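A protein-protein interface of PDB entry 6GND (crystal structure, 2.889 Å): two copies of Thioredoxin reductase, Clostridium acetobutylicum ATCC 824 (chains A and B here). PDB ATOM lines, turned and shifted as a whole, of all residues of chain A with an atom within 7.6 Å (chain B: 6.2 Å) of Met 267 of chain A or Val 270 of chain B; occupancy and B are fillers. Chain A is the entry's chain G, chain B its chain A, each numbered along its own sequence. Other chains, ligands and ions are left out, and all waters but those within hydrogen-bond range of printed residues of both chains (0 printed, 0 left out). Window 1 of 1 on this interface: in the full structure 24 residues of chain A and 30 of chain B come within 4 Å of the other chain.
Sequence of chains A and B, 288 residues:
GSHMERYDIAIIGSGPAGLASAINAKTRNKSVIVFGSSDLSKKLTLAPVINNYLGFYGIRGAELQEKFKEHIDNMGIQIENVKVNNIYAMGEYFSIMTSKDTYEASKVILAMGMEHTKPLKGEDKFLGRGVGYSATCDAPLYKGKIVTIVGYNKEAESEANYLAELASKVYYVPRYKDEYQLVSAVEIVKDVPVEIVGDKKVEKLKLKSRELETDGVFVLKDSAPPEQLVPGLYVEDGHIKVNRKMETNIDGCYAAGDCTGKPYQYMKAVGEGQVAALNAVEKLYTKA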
ATOM      1  N   PRO A  16      14.377 -35.191   3.379  1.00  0.00           N
ATOM      2  CA  PRO A  16      15.374 -34.600   4.290  1.00  0.00           C
ATOM      3  C   PRO A  16      15.089 -34.862   5.761  1.00  0.00           C
ATOM      4  O   PRO A  16      15.999 -35.261   6.499  1.00  0.00           O
ATOM      5  CB  PRO A  16      15.321 -33.106   3.938  1.00  0.00           C
ATOM      6  CG  PRO A  16      14.820 -33.061   2.539  1.00  0.00           C
ATOM      7  CD  PRO A  16      13.891 -34.225   2.377  1.00  0.00           C
ATOM      8  N   ALA A  20      17.583 -36.955   7.927  1.00  0.00           N
ATOM      9  CA  ALA A  20      18.225 -36.314   9.069  1.00  0.00           C
ATOM     10  C   ALA A  20      18.019 -37.130  10.336  1.00  0.00           C
ATOM     11  O   ALA A  20      18.953 -37.315  11.124  1.00  0.00           O
ATOM     12  CB  ALA A  20      17.680 -34.898   9.254  1.00  0.00           C
ATOM     13  N   ILE A  50      19.229 -24.382  -4.821  1.00  0.00           N
ATOM     14  CA  ILE A  50      18.959 -24.047  -3.440  1.00  0.00           C
ATOM     15  C   ILE A  50      19.999 -23.047  -2.959  1.00  0.00           C
ATOM     16  O   ILE A  50      21.195 -23.301  -3.064  1.00  0.00           O
ATOM     17  CB  ILE A  50      18.996 -25.307  -2.570  1.00  0.00           C
ATOM     18  CG1 ILE A  50      18.129 -26.395  -3.200  1.00  0.00           C
ATOM     19  CG2 ILE A  50      18.520 -24.995  -1.164  1.00  0.00           C
ATOM     20  CD1 ILE A  50      18.058 -27.665  -2.385  1.00  0.00           C
ATOM     21  N   ASN A  51      19.559 -21.907  -2.438  1.00  0.00           N
ATOM     22  CA  ASN A  51      20.502 -20.921  -1.931  1.00  0.00           C
ATOM     23  C   ASN A  51      20.349 -20.723  -0.430  1.00  0.00           C
ATOM     24  O   ASN A  51      21.223 -20.157   0.220  1.00  0.00           O
ATOM     25  CB  ASN A  51      20.317 -19.587  -2.653  1.00  0.00           C
ATOM     26  CG  ASN A  51      20.926 -19.586  -4.038  1.00  0.00           C
ATOM     27  OD1 ASN A  51      21.324 -20.628  -4.552  1.00  0.00           O
ATOM     28  ND2 ASN A  51      21.006 -18.412  -4.649  1.00  0.00           N
ATOM     29  N   ASN A  52      19.236 -21.195   0.120  1.00  0.00           N
ATOM     30  CA  ASN A  52      18.980 -21.038   1.544  1.00  0.00           C
ATOM     31  C   ASN A  52      19.332 -22.277   2.365  1.00  0.00           C
ATOM     32  O   ASN A  52      19.045 -22.303   3.565  1.00  0.00           O
ATOM     33  CB  ASN A  52      17.517 -20.645   1.798  1.00  0.00           C
ATOM     34  CG  ASN A  52      16.528 -21.709   1.371  1.00  0.00           C
ATOM     35  OD1 ASN A  52      16.885 -22.859   1.122  1.00  0.00           O
ATOM     36  ND2 ASN A  52      15.256 -21.323   1.307  1.00  0.00           N
ATOM     37  N   TYR A  53      19.922 -23.306   1.763  1.00  0.00           N
ATOM     38  CA  TYR A  53      20.496 -24.401   2.541  1.00  0.00           C
ATOM     39  C   TYR A  53      21.941 -24.036   2.863  1.00  0.00           C
ATOM     40  O   TYR A  53      22.776 -23.936   1.957  1.00  0.00           O
ATOM     41  CB  TYR A  53      20.424 -25.736   1.807  1.00  0.00           C
ATOM     42  CG  TYR A  53      20.663 -26.919   2.726  1.00  0.00           C
ATOM     43  CD1 TYR A  53      21.951 -27.339   3.033  1.00  0.00           C
ATOM     44  CD2 TYR A  53      19.602 -27.586   3.320  1.00  0.00           C
ATOM     45  CE1 TYR A  53      22.172 -28.411   3.882  1.00  0.00           C
ATOM     46  CE2 TYR A  53      19.813 -28.654   4.174  1.00  0.00           C
ATOM     47  CZ  TYR A  53      21.100 -29.063   4.452  1.00  0.00           C
ATOM     48  OH  TYR A  53      21.313 -30.125   5.301  1.00  0.00           O
ATOM     49  N   LEU A  54      22.234 -23.853   4.146  1.00  0.00           N
ATOM     50  CA  LEU A  54      23.508 -23.274   4.547  1.00  0.00           C
ATOM     51  C   LEU A  54      24.652 -24.237   4.267  1.00  0.00           C
ATOM     52  O   LEU A  54      24.626 -25.397   4.689  1.00  0.00           O
ATOM     53  CB  LEU A  54      23.474 -22.886   6.023  1.00  0.00           C
ATOM     54  CG  LEU A  54      24.703 -22.110   6.499  1.00  0.00           C
ATOM     55  CD1 LEU A  54      24.742 -20.722   5.878  1.00  0.00           C
ATOM     56  CD2 LEU A  54      24.702 -21.997   8.016  1.00  0.00           C
ATOM     57  N   GLY A  55      25.663 -23.742   3.554  1.00  0.00           N
ATOM     58  CA  GLY A  55      26.812 -24.522   3.165  1.00  0.00           C
ATOM     59  C   GLY A  55      26.798 -24.979   1.721  1.00  0.00           C
ATOM     60  O   GLY A  55      27.849 -25.374   1.202  1.00  0.00           O
ATOM     61  N   TYR A 264       7.840 -24.782   4.520  1.00  0.00           N
ATOM     62  CA  TYR A 264       8.336 -25.982   3.881  1.00  0.00           C
ATOM     63  C   TYR A 264       9.704 -25.588   3.372  1.00  0.00           C
ATOM     64  O   TYR A 264       9.833 -24.810   2.433  1.00  0.00           O
ATOM     65  CB  TYR A 264       7.432 -26.402   2.728  1.00  0.00           C
ATOM     66  CG  TYR A 264       6.016 -26.723   3.143  1.00  0.00           C
ATOM     67  CD1 TYR A 264       5.751 -27.742   4.043  1.00  0.00           C
ATOM     68  CD2 TYR A 264       4.943 -26.018   2.624  1.00  0.00           C
ATOM     69  CE1 TYR A 264       4.460 -28.043   4.421  1.00  0.00           C
ATOM     70  CE2 TYR A 264       3.648 -26.313   2.997  1.00  0.00           C
ATOM     71  CZ  TYR A 264       3.415 -27.326   3.895  1.00  0.00           C
ATOM     72  OH  TYR A 264       2.130 -27.626   4.272  1.00  0.00           O
ATOM     73  N   GLN A 265      10.729 -26.122   4.014  1.00  0.00           N
ATOM     74  CA  GLN A 265      12.106 -25.812   3.663  1.00  0.00           C
ATOM     75  C   GLN A 265      13.004 -26.965   4.081  1.00  0.00           C
ATOM     76  O   GLN A 265      12.694 -27.703   5.020  1.00  0.00           O
ATOM     77  CB  GLN A 265      12.570 -24.517   4.340  1.00  0.00           C
ATOM     78  CG  GLN A 265      11.919 -23.250   3.808  1.00  0.00           C
ATOM     79  CD  GLN A 265      12.404 -22.866   2.428  1.00  0.00           C
ATOM     80  OE1 GLN A 265      11.934 -21.890   1.849  1.00  0.00           O
ATOM     81  NE2 GLN A 265      13.368 -23.617   1.907  1.00  0.00           N
ATOM     82  N   TYR A 266      14.136 -27.098   3.386  1.00  0.00           N
ATOM     83  CA  TYR A 266      15.044 -28.201   3.675  1.00  0.00           C
ATOM     84  C   TYR A 266      15.587 -28.100   5.094  1.00  0.00           C
ATOM     85  O   TYR A 266      15.552 -29.072   5.856  1.00  0.00           O
ATOM     86  CB  TYR A 266      16.186 -28.247   2.652  1.00  0.00           C
ATOM     87  CG  TYR A 266      15.698 -28.465   1.239  1.00  0.00           C
ATOM     88  CD1 TYR A 266      15.142 -29.681   0.871  1.00  0.00           C
ATOM     89  CD2 TYR A 266      15.852 -27.493   0.260  1.00  0.00           C
ATOM     90  CE1 TYR A 266      14.694 -29.903  -0.411  1.00  0.00           C
ATOM     91  CE2 TYR A 266      15.415 -27.710  -1.036  1.00  0.00           C
ATOM     92  CZ  TYR A 266      14.837 -28.921  -1.364  1.00  0.00           C
ATOM     93  OH  TYR A 266      14.399 -29.155  -2.648  1.00  0.00           O
ATOM     94  N   MET A 267      16.093 -26.924   5.470  1.00  0.00           N
ATOM     95  CA  MET A 267      16.764 -26.792   6.759  1.00  0.00           C
ATOM     96  C   MET A 267      15.802 -26.998   7.926  1.00  0.00           C
ATOM     97  O   MET A 267      16.186 -27.582   8.946  1.00  0.00           O
ATOM     98  CB  MET A 267      17.464 -25.433   6.843  1.00  0.00           C
ATOM     99  CG  MET A 267      18.746 -25.380   6.015  1.00  0.00           C
ATOM    100  SD  MET A 267      19.891 -24.091   6.543  1.00  0.00           S
ATOM    101  CE  MET A 267      18.860 -22.647   6.330  1.00  0.00           C
ATOM    102  N   LYS A 268      14.553 -26.537   7.809  1.00  0.00           N
ATOM    103  CA  LYS A 268      13.578 -26.866   8.844  1.00  0.00           C
ATOM    104  C   LYS A 268      13.353 -28.372   8.905  1.00  0.00           C
ATOM    105  O   LYS A 268      13.293 -28.958   9.992  1.00  0.00           O
ATOM    106  CB  LYS A 268      12.244 -26.156   8.600  1.00  0.00           C
ATOM    107  CG  LYS A 268      11.178 -26.506   9.656  1.00  0.00           C
ATOM    108  CD  LYS A 268       9.786 -26.003   9.306  1.00  0.00           C
ATOM    109  CE  LYS A 268       8.965 -27.060   8.584  1.00  0.00           C
ATOM    110  NZ  LYS A 268       8.629 -28.220   9.443  1.00  0.00           N
ATOM    111  N   ALA A 269      13.223 -29.014   7.740  1.00  0.00           N
ATOM    112  CA  ALA A 269      12.955 -30.446   7.705  1.00  0.00           C
ATOM    113  C   ALA A 269      14.059 -31.231   8.401  1.00  0.00           C
ATOM    114  O   ALA A 269      13.783 -32.111   9.223  1.00  0.00           O
ATOM    115  CB  ALA A 269      12.788 -30.910   6.259  1.00  0.00           C
ATOM    116  N   VAL A 270      15.321 -30.930   8.084  1.00  0.00           N
ATOM    117  CA  VAL A 270      16.423 -31.683   8.677  1.00  0.00           C
ATOM    118  C   VAL A 270      16.517 -31.404  10.172  1.00  0.00           C
ATOM    119  O   VAL A 270      16.706 -32.323  10.977  1.00  0.00           O
ATOM    120  CB  VAL A 270      17.751 -31.373   7.958  1.00  0.00           C
ATOM    121  CG1 VAL A 270      17.651 -31.727   6.479  1.00  0.00           C
ATOM    122  CG2 VAL A 270      18.147 -29.913   8.146  1.00  0.00           C
ATOM    123  N   GLY A 271      16.388 -30.138  10.570  1.00  0.00           N
ATOM    124  CA  GLY A 271      16.388 -29.830  11.987  1.00  0.00           C
ATOM    125  C   GLY A 271      15.313 -30.596  12.732  1.00  0.00           C
ATOM    126  O   GLY A 271      15.574 -31.231  13.755  1.00  0.00           O
ATOM    127  N   GLU A 272      14.082 -30.555  12.216  1.00  0.00           N
ATOM    128  CA  GLU A 272      12.991 -31.284  12.852  1.00  0.00           C
ATOM    129  C   GLU A 272      13.298 -32.774  12.928  1.00  0.00           C
ATOM    130  O   GLU A 272      13.075 -33.410  13.966  1.00  0.00           O
ATOM    131  CB  GLU A 272      11.689 -31.029  12.092  1.00  0.00           C
ATOM    132  CG  GLU A 272      11.106 -29.643  12.349  1.00  0.00           C
ATOM    133  CD  GLU A 272       9.661 -29.509  11.905  1.00  0.00           C
ATOM    134  OE1 GLU A 272       9.095 -30.494  11.378  1.00  0.00           O
ATOM    135  OE2 GLU A 272       9.092 -28.411  12.088  1.00  0.00           O
ATOM    136  N   GLY A 273      13.820 -33.349  11.844  1.00  0.00           N
ATOM    137  CA  GLY A 273      14.170 -34.756  11.871  1.00  0.00           C
ATOM    138  C   GLY A 273      15.198 -35.068  12.940  1.00  0.00           C
ATOM    139  O   GLY A 273      15.107 -36.089  13.628  1.00  0.00           O
ATOM    140  N   GLN A 274      16.193 -34.197  13.091  1.00  0.00           N
ATOM    141  CA  GLN A 274      17.219 -34.417  14.100  1.00  0.00           C
ATOM    142  C   GLN A 274      16.624 -34.407  15.503  1.00  0.00           C
ATOM    143  O   GLN A 274      16.893 -35.302  16.312  1.00  0.00           O
ATOM    144  CB  GLN A 274      18.306 -33.351  13.971  1.00  0.00           C
ATOM    145  CG  GLN A 274      19.387 -33.466  15.021  1.00  0.00           C
ATOM    146  CD  GLN A 274      20.531 -32.515  14.778  1.00  0.00           C
ATOM    147  OE1 GLN A 274      20.325 -31.346  14.458  1.00  0.00           O
ATOM    148  NE2 GLN A 274      21.749 -33.012  14.924  1.00  0.00           N
ATOM    149  N   PRO B  16      25.838 -20.961  13.420  1.00  0.00           N
ATOM    150  CA  PRO B  16      24.957 -21.605  12.428  1.00  0.00           C
ATOM    151  C   PRO B  16      23.561 -21.005  12.400  1.00  0.00           C
ATOM    152  O   PRO B  16      23.036 -20.706  11.321  1.00  0.00           O
ATOM    153  CB  PRO B  16      24.949 -23.074  12.876  1.00  0.00           C
ATOM    154  CG  PRO B  16      26.207 -23.252  13.644  1.00  0.00           C
ATOM    155  CD  PRO B  16      26.499 -21.939  14.303  1.00  0.00           C
ATOM    156  N   ALA B  17      22.942 -20.813  13.566  1.00  0.00           N
ATOM    157  CA  ALA B  17      21.612 -20.217  13.604  1.00  0.00           C
ATOM    158  C   ALA B  17      21.618 -18.830  12.978  1.00  0.00           C
ATOM    159  O   ALA B  17      20.831 -18.542  12.069  1.00  0.00           O
ATOM    160  CB  ALA B  17      21.109 -20.143  15.046  1.00  0.00           C
ATOM    161  N   ALA B  20      22.127 -19.160   9.257  1.00  0.00           N
ATOM    162  CA  ALA B  20      20.939 -19.750   8.648  1.00  0.00           C
ATOM    163  C   ALA B  20      19.797 -18.744   8.611  1.00  0.00           C
ATOM    164  O   ALA B  20      19.094 -18.627   7.601  1.00  0.00           O
ATOM    165  CB  ALA B  20      20.525 -21.011   9.406  1.00  0.00           C
ATOM    166  N   SER B  21      19.599 -18.003   9.705  1.00  0.00           N
ATOM    167  CA  SER B  21      18.610 -16.933   9.699  1.00  0.00           C
ATOM    168  C   SER B  21      18.978 -15.870   8.673  1.00  0.00           C
ATOM    169  O   SER B  21      18.118 -15.387   7.926  1.00  0.00           O
ATOM    170  CB  SER B  21      18.496 -16.301  11.086  1.00  0.00           C
ATOM    171  OG  SER B  21      18.116 -17.245  12.068  1.00  0.00           O
ATOM    172  N   ILE B  23      20.768 -15.897   5.786  1.00  0.00           N
ATOM    173  CA  ILE B  23      20.594 -16.171   4.362  1.00  0.00           C
ATOM    174  C   ILE B  23      19.119 -16.192   3.987  1.00  0.00           C
ATOM    175  O   ILE B  23      18.748 -15.784   2.881  1.00  0.00           O
ATOM    176  CB  ILE B  23      21.281 -17.492   3.954  1.00  0.00           C
ATOM    177  CG1 ILE B  23      20.586 -18.697   4.590  1.00  0.00           C
ATOM    178  CG2 ILE B  23      22.757 -17.463   4.325  1.00  0.00           C
ATOM    179  CD1 ILE B  23      21.260 -20.015   4.262  1.00  0.00           C
ATOM    180  N   ASN B  24      18.254 -16.659   4.890  1.00  0.00           N
ATOM    181  CA  ASN B  24      16.828 -16.675   4.582  1.00  0.00           C
ATOM    182  C   ASN B  24      16.247 -15.267   4.585  1.00  0.00           C
ATOM    183  O   ASN B  24      15.418 -14.933   3.729  1.00  0.00           O
ATOM    184  CB  ASN B  24      16.081 -17.572   5.569  1.00  0.00           C
ATOM    185  CG  ASN B  24      16.211 -19.044   5.224  1.00  0.00           C
ATOM    186  OD1 ASN B  24      15.459 -19.569   4.401  1.00  0.00           O
ATOM    187  ND2 ASN B  24      17.166 -19.717   5.852  1.00  0.00           N
ATOM    188  N   TYR B  53      25.698 -33.784  10.513  1.00  0.00           N
ATOM    189  CA  TYR B  53      25.233 -32.741   9.607  1.00  0.00           C
ATOM    190  C   TYR B  53      25.015 -33.364   8.232  1.00  0.00           C
ATOM    191  O   TYR B  53      25.971 -33.825   7.597  1.00  0.00           O
ATOM    192  CB  TYR B  53      26.228 -31.585   9.513  1.00  0.00           C
ATOM    193  CG  TYR B  53      25.609 -30.326   8.947  1.00  0.00           C
ATOM    194  CD1 TYR B  53      25.429 -30.170   7.582  1.00  0.00           C
ATOM    195  CD2 TYR B  53      25.229 -29.284   9.781  1.00  0.00           C
ATOM    196  CE1 TYR B  53      24.863 -29.022   7.063  1.00  0.00           C
ATOM    197  CE2 TYR B  53      24.667 -28.129   9.273  1.00  0.00           C
ATOM    198  CZ  TYR B  53      24.488 -28.001   7.912  1.00  0.00           C
ATOM    199  OH  TYR B  53      23.928 -26.849   7.402  1.00  0.00           O
ATOM    200  N   PHE B  68      30.331 -22.392   5.163  1.00  0.00           N
ATOM    201  CA  PHE B  68      29.396 -21.362   5.602  1.00  0.00           C
ATOM    202  C   PHE B  68      29.872 -19.961   5.237  1.00  0.00           C
ATOM    203  O   PHE B  68      29.088 -19.122   4.800  1.00  0.00           O
ATOM    204  CB  PHE B  68      29.171 -21.433   7.111  1.00  0.00           C
ATOM    205  CG  PHE B  68      28.450 -22.664   7.561  1.00  0.00           C
ATOM    206  CD1 PHE B  68      27.784 -23.461   6.652  1.00  0.00           C
ATOM    207  CD2 PHE B  68      28.419 -23.009   8.897  1.00  0.00           C
ATOM    208  CE1 PHE B  68      27.116 -24.595   7.066  1.00  0.00           C
ATOM    209  CE2 PHE B  68      27.752 -24.138   9.319  1.00  0.00           C
ATOM    210  CZ  PHE B  68      27.099 -24.932   8.402  1.00  0.00           C
ATOM    211  N   GLY B 257      18.750 -21.506  17.886  1.00  0.00           N
ATOM    212  CA  GLY B 257      20.036 -22.127  18.110  1.00  0.00           C
ATOM    213  C   GLY B 257      20.191 -22.652  19.520  1.00  0.00           C
ATOM    214  O   GLY B 257      19.206 -23.017  20.170  1.00  0.00           O
ATOM    215  N   GLN B 265      22.842 -28.989  18.376  1.00  0.00           N
ATOM    216  CA  GLN B 265      23.360 -29.523  17.138  1.00  0.00           C
ATOM    217  C   GLN B 265      23.250 -28.475  16.050  1.00  0.00           C
ATOM    218  O   GLN B 265      22.447 -27.550  16.135  1.00  0.00           O
ATOM    219  CB  GLN B 265      22.596 -30.777  16.723  1.00  0.00           C
ATOM    220  CG  GLN B 265      22.979 -32.025  17.497  1.00  0.00           C
ATOM    221  CD  GLN B 265      24.454 -32.348  17.394  1.00  0.00           C
ATOM    222  OE1 GLN B 265      24.978 -33.136  18.177  1.00  0.00           O
ATOM    223  NE2 GLN B 265      25.133 -31.741  16.426  1.00  0.00           N
ATOM    224  N   TYR B 266      24.075 -28.631  15.030  1.00  0.00           N
ATOM    225  CA  TYR B 266      24.078 -27.721  13.887  1.00  0.00           C
ATOM    226  C   TYR B 266      22.728 -27.720  13.180  1.00  0.00           C
ATOM    227  O   TYR B 266      22.135 -26.658  12.954  1.00  0.00           O
ATOM    228  CB  TYR B 266      25.192 -28.121  12.917  1.00  0.00           C
ATOM    229  CG  TYR B 266      26.599 -27.989  13.462  1.00  0.00           C
ATOM    230  CD1 TYR B 266      27.277 -26.773  13.449  1.00  0.00           C
ATOM    231  CD2 TYR B 266      27.217 -29.067  14.063  1.00  0.00           C
ATOM    232  CE1 TYR B 266      28.566 -26.665  13.962  1.00  0.00           C
ATOM    233  CE2 TYR B 266      28.484 -28.966  14.594  1.00  0.00           C
ATOM    234  CZ  TYR B 266      29.157 -27.766  14.542  1.00  0.00           C
ATOM    235  OH  TYR B 266      30.426 -27.677  15.073  1.00  0.00           O
ATOM    236  N   MET B 267      22.208 -28.907  12.843  1.00  0.00           N
ATOM    237  CA  MET B 267      21.022 -28.970  11.992  1.00  0.00           C
ATOM    238  C   MET B 267      19.796 -28.378  12.684  1.00  0.00           C
ATOM    239  O   MET B 267      18.979 -27.712  12.035  1.00  0.00           O
ATOM    240  CB  MET B 267      20.756 -30.414  11.556  1.00  0.00           C
ATOM    241  CG  MET B 267      21.745 -30.936  10.522  1.00  0.00           C
ATOM    242  SD  MET B 267      21.103 -32.298   9.524  1.00  0.00           S
ATOM    243  CE  MET B 267      20.674 -33.505  10.781  1.00  0.00           C
ATOM    244  N   LYS B 268      19.629 -28.609  13.990  1.00  0.00           N
ATOM    245  CA  LYS B 268      18.578 -27.896  14.709  1.00  0.00           C
ATOM    246  C   LYS B 268      18.838 -26.397  14.690  1.00  0.00           C
ATOM    247  O   LYS B 268      17.918 -25.600  14.470  1.00  0.00           O
ATOM    248  CB  LYS B 268      18.461 -28.374  16.158  1.00  0.00           C
ATOM    249  CG  LYS B 268      17.484 -27.515  16.986  1.00  0.00           C
ATOM    250  CD  LYS B 268      17.518 -27.835  18.468  1.00  0.00           C
ATOM    251  CE  LYS B 268      18.573 -27.012  19.202  1.00  0.00           C
ATOM    252  NZ  LYS B 268      18.366 -25.543  19.273  1.00  0.00           N
ATOM    253  N   ALA B 269      20.089 -25.998  14.927  1.00  0.00           N
ATOM    254  CA  ALA B 269      20.422 -24.580  14.981  1.00  0.00           C
ATOM    255  C   ALA B 269      20.058 -23.889  13.674  1.00  0.00           C
ATOM    256  O   ALA B 269      19.458 -22.809  13.679  1.00  0.00           O
ATOM    257  CB  ALA B 269      21.904 -24.402  15.299  1.00  0.00           C
ATOM    258  N   VAL B 270      20.416 -24.494  12.538  1.00  0.00           N
ATOM    259  CA  VAL B 270      20.110 -23.859  11.262  1.00  0.00           C
ATOM    260  C   VAL B 270      18.603 -23.828  11.042  1.00  0.00           C
ATOM    261  O   VAL B 270      18.040 -22.806  10.631  1.00  0.00           O
ATOM    262  CB  VAL B 270      20.836 -24.571  10.103  1.00  0.00           C
ATOM    263  CG1 VAL B 270      22.340 -24.567  10.329  1.00  0.00           C
ATOM    264  CG2 VAL B 270      20.321 -25.992   9.906  1.00  0.00           C
ATOM    265  N   GLY B 271      17.923 -24.941  11.325  1.00  0.00           N
ATOM    266  CA  GLY B 271      16.475 -24.960  11.206  1.00  0.00           C
ATOM    267  C   GLY B 271      15.818 -23.898  12.061  1.00  0.00           C
ATOM    268  O   GLY B 271      14.987 -23.120  11.588  1.00  0.00           O
ATOM    269  N   GLU B 272      16.199 -23.838  13.336  1.00  0.00           N
ATOM    270  CA  GLU B 272      15.627 -22.833  14.222  1.00  0.00           C
ATOM    271  C   GLU B 272      15.849 -21.431  13.672  1.00  0.00           C
ATOM    272  O   GLU B 272      14.930 -20.604  13.667  1.00  0.00           O
ATOM    273  CB  GLU B 272      16.217 -22.985  15.628  1.00  0.00           C
ATOM    274  CG  GLU B 272      15.627 -24.176  16.387  1.00  0.00           C
ATOM    275  CD  GLU B 272      15.866 -24.125  17.884  1.00  0.00           C
ATOM    276  OE1 GLU B 272      16.510 -23.166  18.361  1.00  0.00           O
ATOM    277  OE2 GLU B 272      15.389 -25.041  18.588  1.00  0.00           O
ATOM    278  N   GLY B 273      17.058 -21.151  13.183  1.00  0.00           N
ATOM    279  CA  GLY B 273      17.324 -19.848  12.601  1.00  0.00           C
ATOM    280  C   GLY B 273      16.455 -19.550  11.395  1.00  0.00           C
ATOM    281  O   GLY B 273      15.949 -18.434  11.240  1.00  0.00           O
ATOM    282  N   GLN B 274      16.267 -20.540  10.521  1.00  0.00           N
ATOM    283  CA  GLN B 274      15.443 -20.334   9.336  1.00  0.00           C
ATOM    284  C   GLN B 274      14.010 -19.997   9.719  1.00  0.00           C
ATOM    285  O   GLN B 274      13.425 -19.036   9.207  1.00  0.00           O
ATOM    286  CB  GLN B 274      15.470 -21.581   8.458  1.00  0.00           C
ATOM    287  CG  GLN B 274      14.581 -21.483   7.240  1.00  0.00           C
ATOM    288  CD  GLN B 274      14.756 -22.661   6.315  1.00  0.00           C
ATOM    289  OE1 GLN B 274      14.533 -23.808   6.703  1.00  0.00           O
ATOM    290  NE2 GLN B 274      15.169 -22.389   5.083  1.00  0.00           N
ATOM    291  N   VAL B 275      13.427 -20.784  10.625  1.00  0.00           N
ATOM    292  CA  VAL B 275      12.038 -20.560  11.006  1.00  0.00           C
ATOM    293  C   VAL B 275      11.872 -19.157  11.567  1.00  0.00           C
ATOM    294  O   VAL B 275      10.887 -18.468  11.275  1.00  0.00           O
ATOM    295  CB  VAL B 275      11.576 -21.631  12.010  1.00  0.00           C
ATOM    296  CG1 VAL B 275      10.157 -21.341  12.463  1.00  0.00           C
ATOM    297  CG2 VAL B 275      11.656 -23.010  11.380  1.00  0.00           C
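The side-chain hydroxyl (OH) of Tyr 53 of chain B is in hydrogen-bond range of the backbone carbonyl oxygen (O) of Leu 54 of chain A, 3.2 Å away.
The side-chain amide oxygen (OE1) of Gln 274 of chain A lies close to the backbone NH (N) of Met 267 of chain B (3.5 Å).
The backbone NH (N) of Lys 268 of chain B sits at hydrogen-bond distance from the side-chain amide oxygen (OE1) of Gln 274 of chain A, 2.9 Å away.
The backbone NH of Lys 268 of chain A is in hydrogen-bond range of the side-chain amide oxygen of Gln 274 of chain B.
ND2 of Asn 52 of chain A lies close to NE2 of Gln 265 of chain A (3.0 Å).
The side-chain amino group (NZ) of Lys 268 of chain A is in salt-bridge range of the side-chain carboxylate (OE2) of Glu 272 of chain A.
N of Leu 54 of chain A lies within hydrogen-bond range of SD of Met 267 of chain A (3.4 Å).
The backbone carbonyl oxygen (O) of Gly 257 of chain B sits at hydrogen-bond distance from the side-chain amino group (NZ) of Lys 268 of chain B, at 2.8 Å.
Ile 23 of chain B touches Asn 52 of chain A.
Asn 52 of chain A touches Asn 24 of chain B.
Ile 23 of chain B touches Leu 54 of chain A.
Gly 55 of chain A touches Phe 68 of chain B.
Ala 20 of chain B touches Met 267 of chain A (CB to CE, 3.9 Å).
CB of Val 270 of chain B touches SD of Met 267 of chain A, 3.7 Å away.
Met 267 of chain A touches Gly 271 of chain B.
Gly 271 of chain A touches Met 267 of chain B (CA to O, 3.3 Å).
CA of Gly 271 of chain A touches CA of Lys 268 of chain B (3.99 Å).
Of chain B, only Ala 20, Asn 24, Val 270, Gly 271 and Gln 274 come within 4 Å of Met 267 of chain A.
Val 270 of chain B touches one residue of chain A.
Ala 269 of chain B touches none of the printed residues of chain A.
Printed residues of chain B within 4 Å of Gln 274 of chain A: Gln 265 (3.0 Å), Met 267 (3.1 Å) and Lys 268 (2.9 Å).
Printed residues of chain B within 4 Å of Gly 55 of chain A: Phe 68.
Printed residues of chain B within 4 Å of Leu 54 of chain A: Pro 16 (3.9 Å), Ile 23 (3.9 Å), Tyr 53 (3.2 Å) and Phe 68 (3.4 Å).
Of the printed residues of chain A, Val 275 of chain B touches Lys 268.
Ala 17 of chain B touches none of the printed residues of chain A.
The nearest residue of chain B that does not touch Met 267 of chain A is Ile 23 of chain B (4.1 Å).
The nearest residue of chain A that does not touch Val 270 of chain B is Leu 54 of chain A (4.2 Å).
Hydrophobic or aromatic side chains of chain B that line the printed part of chain A: Ala 20, Ile 23, Tyr 53, Phe 68, Met 267, Val 270 and Val 275.
Hydrophobic or aromatic side chains of chain A within 4 Å of the printed part of chain B: Ala 20, Leu 54, Met 267 and Val 270.
Among the printed residues, 23 pairs touch across the chains.
Among the printed residues, no Asp or Glu carboxylate lies within 4 Å of a Lys or Arg side-chain nitrogen of the other chain.
Met 267 of chain A touches Val 270 of chain B, and with the chains exchanged Val 270 of chain A touches Met 267 of chain B.
Met 267 of chain A touches Gly 271 of chain B, and with the chains exchanged Gly 271 of chain A touches Met 267 of chain B.
Lys 268 of chain A touches Gln 274 of chain B, and with the chains exchanged Gln 274 of chain A touches Lys 268 of chain B.
Gly 271 of chain A touches Lys 268 of chain B, but with the chains exchanged Lys 268 of chain A does not touch Gly 271 of chain B (4.2 Å).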
